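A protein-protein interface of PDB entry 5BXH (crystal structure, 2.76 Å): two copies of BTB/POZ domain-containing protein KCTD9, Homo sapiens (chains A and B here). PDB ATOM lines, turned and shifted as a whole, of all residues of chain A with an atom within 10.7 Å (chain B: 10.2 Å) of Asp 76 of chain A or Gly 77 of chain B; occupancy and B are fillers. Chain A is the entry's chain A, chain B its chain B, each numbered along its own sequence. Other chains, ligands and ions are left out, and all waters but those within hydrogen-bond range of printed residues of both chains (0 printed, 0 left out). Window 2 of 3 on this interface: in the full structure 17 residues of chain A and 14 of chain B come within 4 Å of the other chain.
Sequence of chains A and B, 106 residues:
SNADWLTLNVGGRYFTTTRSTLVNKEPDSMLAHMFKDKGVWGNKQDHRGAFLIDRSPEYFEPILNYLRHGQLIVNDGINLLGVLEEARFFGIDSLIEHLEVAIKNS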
ATOM      1  N   TYR A  59      16.128  19.606  25.207  1.00  0.00           N
ATOM      2  CA  TYR A  59      16.089  18.878  23.949  1.00  0.00           C
ATOM      3  C   TYR A  59      15.939  19.831  22.770  1.00  0.00           C
ATOM      4  O   TYR A  59      15.655  19.409  21.652  1.00  0.00           O
ATOM      5  CB  TYR A  59      14.949  17.859  23.954  1.00  0.00           C
ATOM      6  CG  TYR A  59      15.095  16.784  25.009  1.00  0.00           C
ATOM      7  CD1 TYR A  59      15.989  15.735  24.838  1.00  0.00           C
ATOM      8  CD2 TYR A  59      14.337  16.816  26.172  1.00  0.00           C
ATOM      9  CE1 TYR A  59      16.125  14.748  25.796  1.00  0.00           C
ATOM     10  CE2 TYR A  59      14.466  15.833  27.137  1.00  0.00           C
ATOM     11  CZ  TYR A  59      15.362  14.803  26.942  1.00  0.00           C
ATOM     12  OH  TYR A  59      15.498  13.821  27.896  1.00  0.00           O
ATOM     13  N   PRO A  62      20.002  20.425  20.492  1.00  0.00           N
ATOM     14  CA  PRO A  62      20.448  19.753  19.266  1.00  0.00           C
ATOM     15  C   PRO A  62      19.638  20.171  18.041  1.00  0.00           C
ATOM     16  O   PRO A  62      20.138  20.092  16.919  1.00  0.00           O
ATOM     17  CB  PRO A  62      20.232  18.264  19.578  1.00  0.00           C
ATOM     18  CG  PRO A  62      20.031  18.190  21.058  1.00  0.00           C
ATOM     19  CD  PRO A  62      19.365  19.468  21.415  1.00  0.00           C
ATOM     20  N   LEU A  72      23.527  16.074  13.385  1.00  0.00           N
ATOM     21  CA  LEU A  72      22.986  15.557  14.635  1.00  0.00           C
ATOM     22  C   LEU A  72      24.108  15.197  15.603  1.00  0.00           C
ATOM     23  O   LEU A  72      24.782  14.180  15.429  1.00  0.00           O
ATOM     24  CB  LEU A  72      22.109  14.334  14.363  1.00  0.00           C
ATOM     25  CG  LEU A  72      21.579  13.557  15.568  1.00  0.00           C
ATOM     26  CD1 LEU A  72      20.462  14.323  16.262  1.00  0.00           C
ATOM     27  CD2 LEU A  72      21.114  12.170  15.148  1.00  0.00           C
ATOM     28  N   ILE A  73      24.314  16.034  16.617  1.00  0.00           N
ATOM     29  CA  ILE A  73      25.383  15.812  17.589  1.00  0.00           C
ATOM     30  C   ILE A  73      24.894  15.927  19.032  1.00  0.00           C
ATOM     31  O   ILE A  73      24.524  17.011  19.485  1.00  0.00           O
ATOM     32  CB  ILE A  73      26.549  16.808  17.394  1.00  0.00           C
ATOM     33  CG1 ILE A  73      26.982  16.867  15.927  1.00  0.00           C
ATOM     34  CG2 ILE A  73      27.722  16.433  18.289  1.00  0.00           C
ATOM     35  CD1 ILE A  73      28.061  17.893  15.652  1.00  0.00           C
ATOM     36  N   VAL A  74      24.899  14.805  19.749  1.00  0.00           N
ATOM     37  CA  VAL A  74      24.543  14.790  21.167  1.00  0.00           C
ATOM     38  C   VAL A  74      25.535  13.958  21.974  1.00  0.00           C
ATOM     39  O   VAL A  74      26.239  13.110  21.426  1.00  0.00           O
ATOM     40  CB  VAL A  74      23.124  14.232  21.397  1.00  0.00           C
ATOM     41  CG1 VAL A  74      22.075  15.180  20.837  1.00  0.00           C
ATOM     42  CG2 VAL A  74      22.990  12.846  20.785  1.00  0.00           C
ATOM     43  N   ASN A  75      25.582  14.202  23.280  1.00  0.00           N
ATOM     44  CA  ASN A  75      26.485  13.479  24.170  1.00  0.00           C
ATOM     45  C   ASN A  75      25.905  12.133  24.601  1.00  0.00           C
ATOM     46  O   ASN A  75      24.718  11.872  24.398  1.00  0.00           O
ATOM     47  CB  ASN A  75      26.806  14.334  25.396  1.00  0.00           C
ATOM     48  CG  ASN A  75      27.380  15.690  25.026  1.00  0.00           C
ATOM     49  OD1 ASN A  75      28.260  15.790  24.171  1.00  0.00           O
ATOM     50  ND2 ASN A  75      26.878  16.741  25.663  1.00  0.00           N
ATOM     51  N   ASP A  76      26.743  11.283  25.190  1.00  0.00           N
ATOM     52  CA  ASP A  76      26.304   9.963  25.645  1.00  0.00           C
ATOM     53  C   ASP A  76      25.196  10.072  26.682  1.00  0.00           C
ATOM     54  O   ASP A  76      25.217  10.953  27.540  1.00  0.00           O
ATOM     55  CB  ASP A  76      27.472   9.169  26.236  1.00  0.00           C
ATOM     56  CG  ASP A  76      28.501   8.773  25.196  1.00  0.00           C
ATOM     57  OD1 ASP A  76      28.580   9.442  24.144  1.00  0.00           O
ATOM     58  OD2 ASP A  76      29.238   7.794  25.436  1.00  0.00           O
ATOM     59  N   GLY A  77      24.225   9.168  26.596  1.00  0.00           N
ATOM     60  CA  GLY A  77      23.165   9.099  27.581  1.00  0.00           C
ATOM     61  C   GLY A  77      21.946   9.945  27.268  1.00  0.00           C
ATOM     62  O   GLY A  77      20.896   9.776  27.888  1.00  0.00           O
ATOM     63  N   ILE A  78      22.079  10.859  26.313  1.00  0.00           N
ATOM     64  CA  ILE A  78      20.966  11.723  25.936  1.00  0.00           C
ATOM     65  C   ILE A  78      19.884  10.931  25.209  1.00  0.00           C
ATOM     66  O   ILE A  78      20.146  10.299  24.185  1.00  0.00           O
ATOM     67  CB  ILE A  78      21.428  12.893  25.046  1.00  0.00           C
ATOM     68  CG1 ILE A  78      22.402  13.790  25.813  1.00  0.00           C
ATOM     69  CG2 ILE A  78      20.231  13.700  24.565  1.00  0.00           C
ATOM     70  CD1 ILE A  78      22.793  15.051  25.072  1.00  0.00           C
ATOM     71  N   ASN A  79      18.670  10.963  25.749  1.00  0.00           N
ATOM     72  CA  ASN A  79      17.548  10.235  25.167  1.00  0.00           C
ATOM     73  C   ASN A  79      17.111  10.852  23.842  1.00  0.00           C
ATOM     74  O   ASN A  79      16.578  11.961  23.810  1.00  0.00           O
ATOM     75  CB  ASN A  79      16.372  10.198  26.145  1.00  0.00           C
ATOM     76  CG  ASN A  79      15.365   9.114  25.811  1.00  0.00           C
ATOM     77  OD1 ASN A  79      15.316   8.617  24.687  1.00  0.00           O
ATOM     78  ND2 ASN A  79      14.552   8.742  26.793  1.00  0.00           N
ATOM     79  N   LEU A  80      17.331  10.124  22.753  1.00  0.00           N
ATOM     80  CA  LEU A  80      17.069  10.644  21.415  1.00  0.00           C
ATOM     81  C   LEU A  80      15.578  10.874  21.162  1.00  0.00           C
ATOM     82  O   LEU A  80      15.209  11.665  20.293  1.00  0.00           O
ATOM     83  CB  LEU A  80      17.640   9.697  20.358  1.00  0.00           C
ATOM     84  CG  LEU A  80      19.060   9.186  20.618  1.00  0.00           C
ATOM     85  CD1 LEU A  80      19.028   7.758  21.149  1.00  0.00           C
ATOM     86  CD2 LEU A  80      19.920   9.282  19.366  1.00  0.00           C
ATOM     87  N   TYR B  59      29.495  23.141  23.417  1.00  0.00           N
ATOM     88  CA  TYR B  59      30.698  22.669  22.748  1.00  0.00           C
ATOM     89  C   TYR B  59      31.695  23.805  22.544  1.00  0.00           C
ATOM     90  O   TYR B  59      32.712  23.634  21.876  1.00  0.00           O
ATOM     91  CB  TYR B  59      30.347  22.019  21.408  1.00  0.00           C
ATOM     92  CG  TYR B  59      29.481  20.787  21.547  1.00  0.00           C
ATOM     93  CD1 TYR B  59      30.027  19.574  21.948  1.00  0.00           C
ATOM     94  CD2 TYR B  59      28.119  20.834  21.278  1.00  0.00           C
ATOM     95  CE1 TYR B  59      29.242  18.444  22.079  1.00  0.00           C
ATOM     96  CE2 TYR B  59      27.326  19.709  21.407  1.00  0.00           C
ATOM     97  CZ  TYR B  59      27.894  18.517  21.807  1.00  0.00           C
ATOM     98  OH  TYR B  59      27.112  17.393  21.937  1.00  0.00           O
ATOM     99  N   VAL B  74      38.026  17.146  28.382  1.00  0.00           N
ATOM    100  CA  VAL B  74      36.579  16.979  28.318  1.00  0.00           C
ATOM    101  C   VAL B  74      36.109  15.840  29.232  1.00  0.00           C
ATOM    102  O   VAL B  74      36.868  14.918  29.531  1.00  0.00           O
ATOM    103  CB  VAL B  74      36.117  16.718  26.863  1.00  0.00           C
ATOM    104  CG1 VAL B  74      36.340  15.263  26.470  1.00  0.00           C
ATOM    105  CG2 VAL B  74      34.663  17.110  26.681  1.00  0.00           C
ATOM    106  N   ASN B  75      34.860  15.921  29.681  1.00  0.00           N
ATOM    107  CA  ASN B  75      34.292  14.920  30.581  1.00  0.00           C
ATOM    108  C   ASN B  75      33.837  13.663  29.845  1.00  0.00           C
ATOM    109  O   ASN B  75      33.819  13.624  28.615  1.00  0.00           O
ATOM    110  CB  ASN B  75      33.119  15.517  31.361  1.00  0.00           C
ATOM    111  CG  ASN B  75      33.538  16.670  32.254  1.00  0.00           C
ATOM    112  OD1 ASN B  75      34.571  16.609  32.921  1.00  0.00           O
ATOM    113  ND2 ASN B  75      32.739  17.731  32.266  1.00  0.00           N
ATOM    114  N   ASP B  76      33.468  12.637  30.608  1.00  0.00           N
ATOM    115  CA  ASP B  76      33.013  11.375  30.034  1.00  0.00           C
ATOM    116  C   ASP B  76      31.709  11.530  29.265  1.00  0.00           C
ATOM    117  O   ASP B  76      30.816  12.272  29.676  1.00  0.00           O
ATOM    118  CB  ASP B  76      32.832  10.317  31.124  1.00  0.00           C
ATOM    119  CG  ASP B  76      34.137   9.667  31.532  1.00  0.00           C
ATOM    120  OD1 ASP B  76      35.200  10.295  31.353  1.00  0.00           O
ATOM    121  OD2 ASP B  76      34.098   8.524  32.036  1.00  0.00           O
ATOM    122  N   GLY B  77      31.612  10.825  28.144  1.00  0.00           N
ATOM    123  CA  GLY B  77      30.378  10.758  27.388  1.00  0.00           C
ATOM    124  C   GLY B  77      30.117  11.918  26.449  1.00  0.00           C
ATOM    125  O   GLY B  77      29.203  11.857  25.627  1.00  0.00           O
ATOM    126  N   ILE B  78      30.908  12.980  26.561  1.00  0.00           N
ATOM    127  CA  ILE B  78      30.721  14.138  25.694  1.00  0.00           C
ATOM    128  C   ILE B  78      31.209  13.845  24.278  1.00  0.00           C
ATOM    129  O   ILE B  78      32.366  13.476  24.071  1.00  0.00           O
ATOM    130  CB  ILE B  78      31.446  15.383  26.236  1.00  0.00           C
ATOM    131  CG1 ILE B  78      30.801  15.840  27.547  1.00  0.00           C
ATOM    132  CG2 ILE B  78      31.403  16.507  25.213  1.00  0.00           C
ATOM    133  CD1 ILE B  78      31.310  17.172  28.055  1.00  0.00           C
ATOM    134  N   ASN B  79      30.310  14.004  23.312  1.00  0.00           N
ATOM    135  CA  ASN B  79      30.625  13.743  21.914  1.00  0.00           C
ATOM    136  C   ASN B  79      31.683  14.708  21.391  1.00  0.00           C
ATOM    137  O   ASN B  79      31.508  15.925  21.439  1.00  0.00           O
ATOM    138  CB  ASN B  79      29.363  13.834  21.056  1.00  0.00           C
ATOM    139  CG  ASN B  79      29.507  13.119  19.728  1.00  0.00           C
ATOM    140  OD1 ASN B  79      30.616  12.816  19.287  1.00  0.00           O
ATOM    141  ND2 ASN B  79      28.381  12.846  19.079  1.00  0.00           N
ATOM    142  N   LEU B  80      32.779  14.151  20.888  1.00  0.00           N
ATOM    143  CA  LEU B  80      33.908  14.949  20.425  1.00  0.00           C
ATOM    144  C   LEU B  80      33.624  15.576  19.058  1.00  0.00           C
ATOM    145  O   LEU B  80      34.311  16.510  18.636  1.00  0.00           O
ATOM    146  CB  LEU B  80      35.177  14.089  20.365  1.00  0.00           C
ATOM    147  CG  LEU B  80      35.575  13.308  21.626  1.00  0.00           C
ATOM    148  CD1 LEU B  80      34.924  11.926  21.671  1.00  0.00           C
ATOM    149  CD2 LEU B  80      37.090  13.190  21.741  1.00  0.00           C
ATOM    150  N   LEU B  81      32.601  15.062  18.378  1.00  0.00           N
ATOM    151  CA  LEU B  81      32.221  15.556  17.056  1.00  0.00           C
ATOM    152  C   LEU B  81      31.761  17.012  17.084  1.00  0.00           C
ATOM    153  O   LEU B  81      32.072  17.781  16.175  1.00  0.00           O
ATOM    154  CB  LEU B  81      31.117  14.682  16.453  1.00  0.00           C
ATOM    155  CG  LEU B  81      31.558  13.550  15.521  1.00  0.00           C
ATOM    156  CD1 LEU B  81      32.199  12.408  16.298  1.00  0.00           C
ATOM    157  CD2 LEU B  81      30.385  13.052  14.686  1.00  0.00           C
ATOM    158  N   GLY B  82      31.016  17.385  18.120  1.00  0.00           N
ATOM    159  CA  GLY B  82      30.551  18.753  18.265  1.00  0.00           C
ATOM    160  C   GLY B  82      31.709  19.710  18.466  1.00  0.00           C
ATOM    161  O   GLY B  82      31.773  20.775  17.842  1.00  0.00           O
ATOM    162  N   VAL B  83      32.628  19.316  19.343  1.00  0.00           N
ATOM    163  CA  VAL B  83      33.842  20.081  19.593  1.00  0.00           C
ATOM    164  C   VAL B  83      34.635  20.248  18.301  1.00  0.00           C
ATOM    165  O   VAL B  83      35.168  21.323  18.026  1.00  0.00           O
ATOM    166  CB  VAL B  83      34.728  19.404  20.657  1.00  0.00           C
ATOM    167  CG1 VAL B  83      35.850  20.337  21.084  1.00  0.00           C
ATOM    168  CG2 VAL B  83      33.890  18.991  21.856  1.00  0.00           C
ATOM    169  N   SER B 106      38.905   5.740  19.945  1.00  0.00           N
ATOM    170  CA  SER B 106      38.013   6.057  21.055  1.00  0.00           C
ATOM    171  C   SER B 106      37.534   4.789  21.758  1.00  0.00           C
ATOM    172  O   SER B 106      36.742   4.024  21.207  1.00  0.00           O
ATOM    173  CB  SER B 106      36.812   6.871  20.566  1.00  0.00           C
ATOM    174  OG  SER B 106      37.222   8.120  20.038  1.00  0.00           O
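The backbone NH (N) of Asn 79 of chain B lies within hydrogen-bond range of the side-chain amide oxygen (OD1) of Asn 75 of chain A, at 2.9 Å. O of Val 74 of chain A sits at hydrogen-bond distance from ND2 of Asn 79 of chain B. The side-chain amide oxygen of Asn 75 of chain A lies within hydrogen-bond range of the side-chain hydroxyl of Tyr 59 of chain B (3.0 Å). N of Asp 76 of chain A is in hydrogen-bond range of O of Gly 77 of chain B (2.6 Å).
The side-chain amide oxygen of Asn 79 of chain B is in hydrogen-bond range of the backbone NH of Leu 81 of chain B, 3.1 Å away.
Among the printed residues, merely in contact across the chains: Ile 73 of chain A with Tyr 59 of chain B (3.6 Å), Ile 73 of chain A with Asn 79 of chain B (3.7 Å), Ile 73 of chain A with Gly 82 of chain B (3.4 Å), Val 74 of chain A with Tyr 59 of chain B (3.7 Å), Asn 75 of chain A with Gly 77 of chain B (3.5 Å) and Asn 75 of chain A with Ile 78 of chain B (3.3 Å).
Asp 76 of chain A touches just one residue of chain B: Gly 77. Gly 77 of chain B touches just these residues of chain A: Asn 75 (3.5 Å) and Asp 76 (2.6 Å). Of chain B, only Tyr 59 (3.0 Å), Gly 77 (3.5 Å), Ile 78 (3.3 Å) and Asn 79 (2.9 Å) come within 4 Å of Asn 75 of chain A. No residue of chain B comes within 4 Å of Gly 77 of chain A. No residue of chain A comes within 4 Å of Asp 76 of chain B. Of chain A, only Ile 73 (3.7 Å), Val 74 (3.2 Å) and Asn 75 (2.9 Å) come within 4 Å of Asn 79 of chain B. Of the printed residues of chain A, Gly 82 of chain B touches Ile 73. Of the printed residues of chain A, Tyr 59 of chain B touches Ile 73, Val 74 and Asn 75. Leu 81 of chain B touches none of the printed residues of chain A. The nearest residue of chain A that does not touch Gly 77 of chain B is Val 74 of chain A (5.3 Å).
Of the 12 printed residues of chain B, 5 touch a printed residue of chain A. Among the printed residues, 10 pairs touch across the chains.
Val 74 of chain A touches Tyr 59 of chain B, but with the chains exchanged Tyr 59 of chain A does not touch Val 74 of chain B (18.7 Å). Asn 75 of chain A touches Tyr 59 of chain B, but with the chains exchanged Tyr 59 of chain A does not touch Asn 75 of chain B (17.9 Å). Asn 75 of chain A touches Gly 77 of chain B, but with the chains exchanged Gly 77 of chain A does not touch Asn 75 of chain B (10.8 Å). Asp 76 of chain A touches Gly 77 of chain B, but with the chains exchanged Gly 77 of chain A does not touch Asp 76 of chain B (7.9 Å). Of the 10 pairs that touch across the chains among the printed residues, none has its exchanged pair printed and touching as well.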
